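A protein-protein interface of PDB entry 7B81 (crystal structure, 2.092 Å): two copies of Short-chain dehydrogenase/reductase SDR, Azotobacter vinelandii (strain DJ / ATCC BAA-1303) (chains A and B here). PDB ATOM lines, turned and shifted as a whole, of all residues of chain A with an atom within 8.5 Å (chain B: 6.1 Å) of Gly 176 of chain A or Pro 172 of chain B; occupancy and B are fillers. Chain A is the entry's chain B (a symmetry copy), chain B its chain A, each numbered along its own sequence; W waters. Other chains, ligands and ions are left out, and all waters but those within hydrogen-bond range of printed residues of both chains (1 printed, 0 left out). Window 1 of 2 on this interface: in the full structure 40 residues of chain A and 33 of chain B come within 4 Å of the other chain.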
ATOM      1  N   ASN A 128     -21.401  19.249  21.760  1.00  0.00           N
ATOM      2  CA  ASN A 128     -22.249  20.131  20.969  1.00  0.00           C
ATOM      3  C   ASN A 128     -21.469  21.221  20.250  1.00  0.00           C
ATOM      4  O   ASN A 128     -21.863  21.628  19.147  1.00  0.00           O
ATOM      5  CB  ASN A 128     -23.314  20.771  21.866  1.00  0.00           C
ATOM      6  CG  ASN A 128     -24.137  19.742  22.624  1.00  0.00           C
ATOM      7  OD1 ASN A 128     -23.816  18.551  22.627  1.00  0.00           O
ATOM      8  ND2 ASN A 128     -25.203  20.198  23.270  1.00  0.00           N
ATOM      9  N   LEU A 129     -20.379  21.706  20.840  1.00  0.00           N
ATOM     10  CA  LEU A 129     -19.595  22.787  20.252  1.00  0.00           C
ATOM     11  C   LEU A 129     -18.267  22.240  19.738  1.00  0.00           C
ATOM     12  O   LEU A 129     -18.051  22.192  18.524  1.00  0.00           O
ATOM     13  CB  LEU A 129     -19.385  23.904  21.279  1.00  0.00           C
ATOM     14  CG  LEU A 129     -19.074  25.349  20.855  1.00  0.00           C
ATOM     15  CD1 LEU A 129     -18.822  26.209  22.091  1.00  0.00           C
ATOM     16  CD2 LEU A 129     -17.939  25.492  19.855  1.00  0.00           C
ATOM     17  N   ASN A 130     -17.381  21.786  20.636  1.00  0.00           N
ATOM     18  CA  ASN A 130     -16.012  21.441  20.252  1.00  0.00           C
ATOM     19  C   ASN A 130     -15.985  20.351  19.189  1.00  0.00           C
ATOM     20  O   ASN A 130     -15.264  20.461  18.190  1.00  0.00           O
ATOM     21  CB  ASN A 130     -15.221  21.013  21.488  1.00  0.00           C
ATOM     22  CG  ASN A 130     -15.132  22.112  22.532  1.00  0.00           C
ATOM     23  OD1 ASN A 130     -15.708  23.185  22.369  1.00  0.00           O
ATOM     24  ND2 ASN A 130     -14.409  21.846  23.614  1.00  0.00           N
ATOM     25  N   ALA A 132     -18.379  19.655  17.141  1.00  0.00           N
ATOM     26  CA  ALA A 132     -18.945  20.215  15.920  1.00  0.00           C
ATOM     27  C   ALA A 132     -17.919  21.057  15.172  1.00  0.00           C
ATOM     28  O   ALA A 132     -17.880  21.033  13.937  1.00  0.00           O
ATOM     29  CB  ALA A 132     -20.186  21.042  16.247  1.00  0.00           C
ATOM     30  N   TYR A 133     -17.070  21.790  15.901  1.00  0.00           N
ATOM     31  CA  TYR A 133     -16.120  22.695  15.256  1.00  0.00           C
ATOM     32  C   TYR A 133     -15.157  21.943  14.348  1.00  0.00           C
ATOM     33  O   TYR A 133     -14.752  22.458  13.299  1.00  0.00           O
ATOM     34  CB  TYR A 133     -15.341  23.487  16.308  1.00  0.00           C
ATOM     35  CG  TYR A 133     -14.343  24.475  15.726  1.00  0.00           C
ATOM     36  CD1 TYR A 133     -13.053  24.078  15.379  1.00  0.00           C
ATOM     37  CD2 TYR A 133     -14.687  25.805  15.529  1.00  0.00           C
ATOM     38  CE1 TYR A 133     -12.144  24.974  14.848  1.00  0.00           C
ATOM     39  CE2 TYR A 133     -13.781  26.711  15.000  1.00  0.00           C
ATOM     40  CZ  TYR A 133     -12.512  26.287  14.661  1.00  0.00           C
ATOM     41  OH  TYR A 133     -11.608  27.182  14.134  1.00  0.00           O
ATOM     42  N   ALA A 154     -25.919  23.534  10.588  1.00  0.00           N
ATOM     43  CA  ALA A 154     -25.782  23.192  11.997  1.00  0.00           C
ATOM     44  C   ALA A 154     -27.149  23.255  12.667  1.00  0.00           C
ATOM     45  O   ALA A 154     -27.870  24.247  12.525  1.00  0.00           O
ATOM     46  CB  ALA A 154     -24.801  24.132  12.699  1.00  0.00           C
ATOM     47  N   SER A 156     -28.708  24.024  15.718  1.00  0.00           N
ATOM     48  CA  SER A 156     -28.648  24.610  17.049  1.00  0.00           C
ATOM     49  C   SER A 156     -30.077  24.652  17.584  1.00  0.00           C
ATOM     50  O   SER A 156     -30.852  23.728  17.312  1.00  0.00           O
ATOM     51  CB  SER A 156     -27.961  25.978  17.022  1.00  0.00           C
ATOM     52  OG  SER A 156     -28.879  27.049  17.039  1.00  0.00           O
ATOM     53  N   SER A 157     -30.459  25.690  18.325  1.00  0.00           N
ATOM     54  CA  SER A 157     -31.747  25.664  19.007  1.00  0.00           C
ATOM     55  C   SER A 157     -32.388  27.044  19.030  1.00  0.00           C
ATOM     56  O   SER A 157     -31.727  28.065  18.845  1.00  0.00           O
ATOM     57  CB  SER A 157     -31.614  25.149  20.447  1.00  0.00           C
ATOM     58  OG  SER A 157     -32.779  25.454  21.197  1.00  0.00           O
ATOM     59  N   SER A 159     -33.114  28.076  21.731  1.00  0.00           N
ATOM     60  CA  SER A 159     -32.341  28.527  22.879  1.00  0.00           C
ATOM     61  C   SER A 159     -31.055  29.238  22.488  1.00  0.00           C
ATOM     62  O   SER A 159     -30.338  29.705  23.378  1.00  0.00           O
ATOM     63  CB  SER A 159     -32.017  27.342  23.789  1.00  0.00           C
ATOM     64  OG  SER A 159     -33.126  26.469  23.903  1.00  0.00           O
ATOM     65  N   ALA A 160     -30.729  29.319  21.194  1.00  0.00           N
ATOM     66  CA  ALA A 160     -29.656  30.206  20.766  1.00  0.00           C
ATOM     67  C   ALA A 160     -30.078  31.666  20.836  1.00  0.00           C
ATOM     68  O   ALA A 160     -29.214  32.550  20.812  1.00  0.00           O
ATOM     69  CB  ALA A 160     -29.209  29.861  19.344  1.00  0.00           C
ATOM     70  N   TYR A 170     -26.037  24.416  28.202  1.00  0.00           N
ATOM     71  CA  TYR A 170     -26.539  23.998  26.899  1.00  0.00           C
ATOM     72  C   TYR A 170     -26.691  25.164  25.930  1.00  0.00           C
ATOM     73  O   TYR A 170     -26.147  25.120  24.821  1.00  0.00           O
ATOM     74  CB  TYR A 170     -27.880  23.273  27.078  1.00  0.00           C
ATOM     75  CG  TYR A 170     -28.601  22.938  25.790  1.00  0.00           C
ATOM     76  CD1 TYR A 170     -28.178  21.891  24.982  1.00  0.00           C
ATOM     77  CD2 TYR A 170     -29.719  23.661  25.391  1.00  0.00           C
ATOM     78  CE1 TYR A 170     -28.842  21.582  23.805  1.00  0.00           C
ATOM     79  CE2 TYR A 170     -30.389  23.360  24.220  1.00  0.00           C
ATOM     80  CZ  TYR A 170     -29.947  22.321  23.432  1.00  0.00           C
ATOM     81  OH  TYR A 170     -30.616  22.022  22.267  1.00  0.00           O
ATOM     82  N   THR A 171     -27.402  26.217  26.334  1.00  0.00           N
ATOM     83  CA  THR A 171     -27.664  27.324  25.416  1.00  0.00           C
ATOM     84  C   THR A 171     -26.404  27.993  24.865  1.00  0.00           C
ATOM     85  O   THR A 171     -26.438  28.415  23.695  1.00  0.00           O
ATOM     86  CB  THR A 171     -28.587  28.357  26.083  1.00  0.00           C
ATOM     87  OG1 THR A 171     -27.904  29.027  27.150  1.00  0.00           O
ATOM     88  CG2 THR A 171     -29.841  27.682  26.633  1.00  0.00           C
ATOM     89  N   PRO A 172     -25.291  28.133  25.602  1.00  0.00           N
ATOM     90  CA  PRO A 172     -24.099  28.731  24.974  1.00  0.00           C
ATOM     91  C   PRO A 172     -23.526  27.888  23.854  1.00  0.00           C
ATOM     92  O   PRO A 172     -22.981  28.446  22.893  1.00  0.00           O
ATOM     93  CB  PRO A 172     -23.111  28.864  26.141  1.00  0.00           C
ATOM     94  CG  PRO A 172     -23.968  28.871  27.358  1.00  0.00           C
ATOM     95  CD  PRO A 172     -25.066  27.913  27.042  1.00  0.00           C
ATOM     96  N   THR A 173     -23.622  26.560  23.949  1.00  0.00           N
ATOM     97  CA  THR A 173     -23.157  25.717  22.852  1.00  0.00           C
ATOM     98  C   THR A 173     -24.034  25.895  21.617  1.00  0.00           C
ATOM     99  O   THR A 173     -23.535  25.871  20.485  1.00  0.00           O
ATOM    100  CB  THR A 173     -23.122  24.249  23.287  1.00  0.00           C
ATOM    101  OG1 THR A 173     -24.444  23.697  23.256  1.00  0.00           O
ATOM    102  CG2 THR A 173     -22.556  24.121  24.697  1.00  0.00           C
ATOM    103  N   LYS A 174     -25.338  26.099  21.816  1.00  0.00           N
ATOM    104  CA  LYS A 174     -26.241  26.299  20.686  1.00  0.00           C
ATOM    105  C   LYS A 174     -26.080  27.692  20.085  1.00  0.00           C
ATOM    106  O   LYS A 174     -26.135  27.855  18.860  1.00  0.00           O
ATOM    107  CB  LYS A 174     -27.690  26.066  21.119  1.00  0.00           C
ATOM    108  CG  LYS A 174     -27.892  24.859  22.030  1.00  0.00           C
ATOM    109  CD  LYS A 174     -27.215  23.604  21.480  1.00  0.00           C
ATOM    110  CE  LYS A 174     -27.942  23.053  20.271  1.00  0.00           C
ATOM    111  NZ  LYS A 174     -27.226  21.869  19.724  1.00  0.00           N
ATOM    112  N   ALA A 175     -25.888  28.707  20.930  1.00  0.00           N
ATOM    113  CA  ALA A 175     -25.572  30.030  20.412  1.00  0.00           C
ATOM    114  C   ALA A 175     -24.187  30.057  19.780  1.00  0.00           C
ATOM    115  O   ALA A 175     -23.945  30.841  18.857  1.00  0.00           O
ATOM    116  CB  ALA A 175     -25.675  31.072  21.524  1.00  0.00           C
ATOM    117  N   GLY A 176     -23.275  29.204  20.254  1.00  0.00           N
ATOM    118  CA  GLY A 176     -21.972  29.090  19.624  1.00  0.00           C
ATOM    119  C   GLY A 176     -22.021  28.396  18.277  1.00  0.00           C
ATOM    120  O   GLY A 176     -21.228  28.711  17.385  1.00  0.00           O
ATOM    121  N   LEU A 177     -22.940  27.442  18.112  1.00  0.00           N
ATOM    122  CA  LEU A 177     -23.134  26.805  16.813  1.00  0.00           C
ATOM    123  C   LEU A 177     -23.641  27.803  15.783  1.00  0.00           C
ATOM    124  O   LEU A 177     -23.206  27.790  14.626  1.00  0.00           O
ATOM    125  CB  LEU A 177     -24.117  25.642  16.939  1.00  0.00           C
ATOM    126  CG  LEU A 177     -23.566  24.285  17.363  1.00  0.00           C
ATOM    127  CD1 LEU A 177     -24.639  23.228  17.190  1.00  0.00           C
ATOM    128  CD2 LEU A 177     -22.333  23.938  16.555  1.00  0.00           C
ATOM    129  N   LEU A 178     -24.585  28.659  16.182  1.00  0.00           N
ATOM    130  CA  LEU A 178     -25.045  29.729  15.305  1.00  0.00           C
ATOM    131  C   LEU A 178     -23.888  30.635  14.907  1.00  0.00           C
ATOM    132  O   LEU A 178     -23.647  30.870  13.718  1.00  0.00           O
ATOM    133  CB  LEU A 178     -26.143  30.531  16.003  1.00  0.00           C
ATOM    134  CG  LEU A 178     -27.215  31.190  15.135  1.00  0.00           C
ATOM    135  CD1 LEU A 178     -28.440  31.521  15.980  1.00  0.00           C
ATOM    136  CD2 LEU A 178     -26.677  32.439  14.454  1.00  0.00           C
ATOM    137  N   SER A 179     -23.153  31.142  15.898  1.00  0.00           N
ATOM    138  CA  SER A 179     -22.044  32.048  15.625  1.00  0.00           C
ATOM    139  C   SER A 179     -20.983  31.382  14.761  1.00  0.00           C
ATOM    140  O   SER A 179     -20.360  32.036  13.914  1.00  0.00           O
ATOM    141  CB  SER A 179     -21.445  32.531  16.944  1.00  0.00           C
ATOM    142  OG  SER A 179     -20.120  32.985  16.781  1.00  0.00           O
ATOM    143  N   LEU A 180     -20.762  30.081  14.961  1.00  0.00           N
ATOM    144  CA  LEU A 180     -19.831  29.341  14.115  1.00  0.00           C
ATOM    145  C   LEU A 180     -20.246  29.413  12.652  1.00  0.00           C
ATOM    146  O   LEU A 180     -19.425  29.711  11.774  1.00  0.00           O
ATOM    147  CB  LEU A 180     -19.745  27.887  14.578  1.00  0.00           C
ATOM    148  CG  LEU A 180     -18.702  27.052  13.837  1.00  0.00           C
ATOM    149  CD1 LEU A 180     -17.320  27.618  14.088  1.00  0.00           C
ATOM    150  CD2 LEU A 180     -18.780  25.594  14.256  1.00  0.00           C
ATOM    151  N   MET A 181     -21.526  29.156  12.371  1.00  0.00           N
ATOM    152  CA  MET A 181     -22.020  29.261  11.002  1.00  0.00           C
ATOM    153  C   MET A 181     -21.881  30.678  10.456  1.00  0.00           C
ATOM    154  O   MET A 181     -21.681  30.861   9.249  1.00  0.00           O
ATOM    155  CB  MET A 181     -23.479  28.807  10.937  1.00  0.00           C
ATOM    156  CG  MET A 181     -23.710  27.350  11.322  1.00  0.00           C
ATOM    157  SD  MET A 181     -22.905  26.165  10.223  1.00  0.00           S
ATOM    158  CE  MET A 181     -21.400  25.827  11.143  1.00  0.00           C
ATOM    159  N   GLN A 182     -21.980  31.691  11.320  1.00  0.00           N
ATOM    160  CA  GLN A 182     -21.820  33.067  10.858  1.00  0.00           C
ATOM    161  C   GLN A 182     -20.381  33.339  10.437  1.00  0.00           C
ATOM    162  O   GLN A 182     -20.132  33.886   9.355  1.00  0.00           O
ATOM    163  CB  GLN A 182     -22.263  34.046  11.950  1.00  0.00           C
ATOM    164  CG  GLN A 182     -23.701  33.823  12.425  1.00  0.00           C
ATOM    165  CD  GLN A 182     -24.152  34.853  13.436  1.00  0.00           C
ATOM    166  OE1 GLN A 182     -23.491  35.074  14.451  1.00  0.00           O
ATOM    167  NE2 GLN A 182     -25.284  35.493  13.162  1.00  0.00           N
ATOM    168  N   SER A 183     -19.413  32.965  11.280  1.00  0.00           N
ATOM    169  CA  SER A 183     -18.017  33.192  10.916  1.00  0.00           C
ATOM    170  C   SER A 183     -17.564  32.241   9.815  1.00  0.00           C
ATOM    171  O   SER A 183     -16.848  32.652   8.897  1.00  0.00           O
ATOM    172  CB  SER A 183     -17.115  33.073  12.141  1.00  0.00           C
ATOM    173  OG  SER A 183     -17.553  33.931  13.178  1.00  0.00           O
ATOM    174  N   CYS A 184     -17.978  30.973   9.874  1.00  0.00           N
ATOM    175  CA  CYS A 184     -17.614  30.051   8.802  1.00  0.00           C
ATOM    176  C   CYS A 184     -18.200  30.496   7.468  1.00  0.00           C
ATOM    177  O   CYS A 184     -17.604  30.245   6.417  1.00  0.00           O
ATOM    178  CB  CYS A 184     -18.060  28.629   9.136  1.00  0.00           C
ATOM    179  SG  CYS A 184     -17.041  27.817  10.385  1.00  0.00           S
ATOM    180  N   ALA A 197     -27.753  27.702   9.906  1.00  0.00           N
ATOM    181  CA  ALA A 197     -28.204  27.022  11.106  1.00  0.00           C
ATOM    182  C   ALA A 197     -29.719  26.948  11.111  1.00  0.00           C
ATOM    183  O   ALA A 197     -30.398  27.915  10.751  1.00  0.00           O
ATOM    184  CB  ALA A 197     -27.706  27.733  12.366  1.00  0.00           C
ATOM    185  N   LEU B 129     -14.992  31.077  27.605  1.00  0.00           N
ATOM    186  CA  LEU B 129     -16.302  30.520  27.917  1.00  0.00           C
ATOM    187  C   LEU B 129     -16.273  29.613  29.140  1.00  0.00           C
ATOM    188  O   LEU B 129     -16.962  29.890  30.127  1.00  0.00           O
ATOM    189  CB  LEU B 129     -16.846  29.763  26.698  1.00  0.00           C
ATOM    190  CG  LEU B 129     -18.315  29.352  26.779  1.00  0.00           C
ATOM    191  CD1 LEU B 129     -19.193  30.563  27.064  1.00  0.00           C
ATOM    192  CD2 LEU B 129     -18.744  28.658  25.498  1.00  0.00           C
ATOM    193  N   SER B 159     -19.169  40.774  17.847  1.00  0.00           N
ATOM    194  CA  SER B 159     -18.990  39.480  17.199  1.00  0.00           C
ATOM    195  C   SER B 159     -19.925  38.405  17.743  1.00  0.00           C
ATOM    196  O   SER B 159     -19.909  37.281  17.233  1.00  0.00           O
ATOM    197  CB  SER B 159     -17.541  39.011  17.351  1.00  0.00           C
ATOM    198  OG  SER B 159     -16.637  39.905  16.715  1.00  0.00           O
ATOM    199  N   GLN B 167     -11.867  34.557  13.218  1.00  0.00           N
ATOM    200  CA  GLN B 167     -12.338  34.423  14.591  1.00  0.00           C
ATOM    201  C   GLN B 167     -13.376  33.313  14.718  1.00  0.00           C
ATOM    202  O   GLN B 167     -14.249  33.377  15.587  1.00  0.00           O
ATOM    203  CB  GLN B 167     -12.922  35.740  15.103  1.00  0.00           C
ATOM    204  CG  GLN B 167     -12.037  36.957  14.912  1.00  0.00           C
ATOM    205  CD  GLN B 167     -12.774  38.247  15.189  1.00  0.00           C
ATOM    206  OE1 GLN B 167     -13.673  38.632  14.442  1.00  0.00           O
ATOM    207  NE2 GLN B 167     -12.404  38.920  16.270  1.00  0.00           N
ATOM    208  N   THR B 168     -13.304  32.291  13.858  1.00  0.00           N
ATOM    209  CA  THR B 168     -14.228  31.166  13.960  1.00  0.00           C
ATOM    210  C   THR B 168     -14.094  30.434  15.288  1.00  0.00           C
ATOM    211  O   THR B 168     -15.043  29.775  15.722  1.00  0.00           O
ATOM    212  CB  THR B 168     -14.014  30.182  12.804  1.00  0.00           C
ATOM    213  OG1 THR B 168     -12.760  29.507  12.969  1.00  0.00           O
ATOM    214  CG2 THR B 168     -14.021  30.909  11.467  1.00  0.00           C
ATOM    215  N   HIS B 169     -12.935  30.532  15.938  1.00  0.00           N
ATOM    216  CA  HIS B 169     -12.737  29.987  17.274  1.00  0.00           C
ATOM    217  C   HIS B 169     -13.125  30.968  18.369  1.00  0.00           C
ATOM    218  O   HIS B 169     -13.306  30.555  19.520  1.00  0.00           O
ATOM    219  CB  HIS B 169     -11.272  29.580  17.463  1.00  0.00           C
ATOM    220  CG  HIS B 169     -10.313  30.730  17.395  1.00  0.00           C
ATOM    221  ND1 HIS B 169     -10.214  31.552  16.293  1.00  0.00           N
ATOM    222  CD2 HIS B 169      -9.411  31.196  18.292  1.00  0.00           C
ATOM    223  CE1 HIS B 169      -9.289  32.471  16.511  1.00  0.00           C
ATOM    224  NE2 HIS B 169      -8.790  32.279  17.718  1.00  0.00           N
ATOM    225  N   TYR B 170     -13.267  32.249  18.030  1.00  0.00           N
ATOM    226  CA  TYR B 170     -13.470  33.322  18.994  1.00  0.00           C
ATOM    227  C   TYR B 170     -14.933  33.726  19.135  1.00  0.00           C
ATOM    228  O   TYR B 170     -15.439  33.828  20.257  1.00  0.00           O
ATOM    229  CB  TYR B 170     -12.618  34.530  18.583  1.00  0.00           C
ATOM    230  CG  TYR B 170     -12.890  35.806  19.343  1.00  0.00           C
ATOM    231  CD1 TYR B 170     -12.454  35.967  20.653  1.00  0.00           C
ATOM    232  CD2 TYR B 170     -13.557  36.865  18.739  1.00  0.00           C
ATOM    233  CE1 TYR B 170     -12.690  37.145  21.344  1.00  0.00           C
ATOM    234  CE2 TYR B 170     -13.798  38.044  19.421  1.00  0.00           C
ATOM    235  CZ  TYR B 170     -13.363  38.178  20.721  1.00  0.00           C
ATOM    236  OH  TYR B 170     -13.603  39.353  21.395  1.00  0.00           O
ATOM    237  N   THR B 171     -15.628  33.953  18.021  1.00  0.00           N
ATOM    238  CA  THR B 171     -17.005  34.425  18.109  1.00  0.00           C
ATOM    239  C   THR B 171     -17.961  33.444  18.792  1.00  0.00           C
ATOM    240  O   THR B 171     -18.906  33.925  19.442  1.00  0.00           O
ATOM    241  CB  THR B 171     -17.536  34.808  16.715  1.00  0.00           C
ATOM    242  OG1 THR B 171     -17.909  33.633  15.984  1.00  0.00           O
ATOM    243  CG2 THR B 171     -16.496  35.601  15.923  1.00  0.00           C
ATOM    244  N   PRO B 172     -17.807  32.114  18.697  1.00  0.00           N
ATOM    245  CA  PRO B 172     -18.685  31.245  19.500  1.00  0.00           C
ATOM    246  C   PRO B 172     -18.539  31.455  20.994  1.00  0.00           C
ATOM    247  O   PRO B 172     -19.527  31.331  21.728  1.00  0.00           O
ATOM    248  CB  PRO B 172     -18.256  29.831  19.084  1.00  0.00           C
ATOM    249  CG  PRO B 172     -17.712  30.003  17.718  1.00  0.00           C
ATOM    250  CD  PRO B 172     -16.995  31.315  17.760  1.00  0.00           C
ATOM    251  N   THR B 173     -17.334  31.773  21.474  1.00  0.00           N
ATOM    252  CA  THR B 173     -17.165  31.998  22.904  1.00  0.00           C
ATOM    253  C   THR B 173     -17.894  33.257  23.349  1.00  0.00           C
ATOM    254  O   THR B 173     -18.474  33.289  24.441  1.00  0.00           O
ATOM    255  CB  THR B 173     -15.681  32.082  23.261  1.00  0.00           C
ATOM    256  OG1 THR B 173     -15.121  33.283  22.714  1.00  0.00           O
ATOM    257  CG2 THR B 173     -14.933  30.871  22.711  1.00  0.00           C
ATOM    258  N   LYS B 174     -17.889  34.299  22.514  1.00  0.00           N
ATOM    259  CA  LYS B 174     -18.591  35.527  22.877  1.00  0.00           C
ATOM    260  C   LYS B 174     -20.099  35.357  22.734  1.00  0.00           C
ATOM    261  O   LYS B 174     -20.868  35.847  23.570  1.00  0.00           O
ATOM    262  CB  LYS B 174     -18.093  36.696  22.025  1.00  0.00           C
ATOM    263  CG  LYS B 174     -16.594  36.679  21.731  1.00  0.00           C
ATOM    264  CD  LYS B 174     -15.755  36.569  23.002  1.00  0.00           C
ATOM    265  CE  LYS B 174     -15.924  37.777  23.904  1.00  0.00           C
ATOM    266  NZ  LYS B 174     -15.080  37.669  25.130  1.00  0.00           N
ATOM    267  N   ALA B 175     -20.541  34.657  21.687  1.00  0.00           N
ATOM    268  CA  ALA B 175     -21.966  34.385  21.541  1.00  0.00           C
ATOM    269  C   ALA B 175     -22.462  33.470  22.655  1.00  0.00           C
ATOM    270  O   ALA B 175     -23.583  33.635  23.149  1.00  0.00           O
ATOM    271  CB  ALA B 175     -22.247  33.778  20.167  1.00  0.00           C
ATOM    272  N   GLY B 176     -21.639  32.501  23.064  1.00  0.00           N
ATOM    273  CA  GLY B 176     -21.973  31.698  24.226  1.00  0.00           C
ATOM    274  C   GLY B 176     -21.961  32.496  25.515  1.00  0.00           C
ATOM    275  O   GLY B 176     -22.736  32.209  26.434  1.00  0.00           O
ATOM    276  N   LEU B 177     -21.086  33.500  25.603  1.00  0.00           N
ATOM    277  CA  LEU B 177     -21.105  34.413  26.741  1.00  0.00           C
ATOM    278  C   LEU B 177     -22.422  35.172  26.811  1.00  0.00           C
ATOM    279  O   LEU B 177     -22.981  35.368  27.898  1.00  0.00           O
ATOM    280  CB  LEU B 177     -19.937  35.394  26.644  1.00  0.00           C
ATOM    281  CG  LEU B 177     -18.628  35.008  27.326  1.00  0.00           C
ATOM    282  CD1 LEU B 177     -17.695  36.207  27.361  1.00  0.00           C
ATOM    283  CD2 LEU B 177     -18.899  34.496  28.723  1.00  0.00           C
HETATM  284  O   HOH W   1     -21.626  35.702  16.327  1.00  0.00           O
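OH of Tyr 133 of chain A lies within hydrogen-bond range of OG1 of Thr 168 of chain B (2.8 Å).
The side-chain hydroxyl (OG1) of Thr 171 of chain B lies within hydrogen-bond range of the side-chain hydroxyl (OG) of Ser 179 of chain A, at 2.4 Å.
The side-chain hydroxyl (OG1) of Thr 171 of chain B sits at hydrogen-bond distance from the side-chain hydroxyl (OG) of Ser 183 of chain A (2.8 Å).
OG of Ser 179 of chain A lies close to N of Pro 172 of chain B, at 3.1 Å.
The side-chain hydroxyl (OG) of Ser 183 of chain A sits at hydrogen-bond distance from the backbone carbonyl oxygen (O) of Ser 179 of chain A, at 3.5 Å.
O of Leu 180 of chain A lies close to SG of Cys 184 of chain A.
O of Gly 176 of chain B touches CB of Pro 172 of chain A, 3.4 Å away.
Ala 175 of chain A touches Ala 175 of chain B (O to CB, 3.6 Å).
Pro 172 of chain B touches Gly 176 of chain A.
Ser 179 of chain A touches Ala 175 of chain B (CB to CB, 3.5 Å).
Leu 180 of chain A touches Thr 168 of chain B (CD1 to O, 3.5 Å).
Thr 168 of chain B touches Ser 183 of chain A (CG2 to CB, 3.8 Å).
Printed residues of chain B within 4 Å of Gly 176 of chain A: Pro 172.
Of chain A, only Gly 176 and Ser 179 come within 4 Å of Pro 172 of chain B.
Printed residues of chain A within 4 Å of Thr 171 of chain B: Ser 179 (2.4 Å) and Ser 183 (2.8 Å).
Of the printed residues of chain B, Pro 172 of chain A touches Gly 176.
Of the printed residues of chain B, Ala 175 of chain A touches Ala 175.
Of the printed residues of chain B, Ser 183 of chain A touches Thr 168 (3.8 Å) and Thr 171 (2.8 Å).
Thr 171 of chain A touches none of the printed residues of chain B.
Leu 177 of chain B touches none of the printed residues of chain A.
The nearest residue of chain B that does not touch Gly 176 of chain A is Gly 176 of chain B (4.6 Å).
The nearest printed residue of chain A that does not touch Ala 175 of chain B is Gly 176 of chain A (4.7 Å).
Hydrophobic or aromatic side chains of chain A that line the printed part of chain B: Tyr 133, Pro 172, Ala 175 and Leu 180.
Among the printed residues, 10 pairs touch across the chains.
Pro 172 of chain A touches Gly 176 of chain B, and with the chains exchanged Gly 176 of chain A touches Pro 172 of chain B.
Ala 175 of chain A touches its own counterpart, Ala 175 of chain B.
Positions printed for both chains: 129, 159, 170, 171, 172, 173, 174, 175, 176 and 177.
Of the 10 pairs that touch across the chains among the printed residues, 3 have their exchanged pair printed and touching as well.
Water W1 lies within hydrogen-bond range of O of Ser 159 of chain B (2.5 Å), OE1 of Gln 182 of chain A (2.7 Å) and OG of Ser 179 of chain A (3.1 Å).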
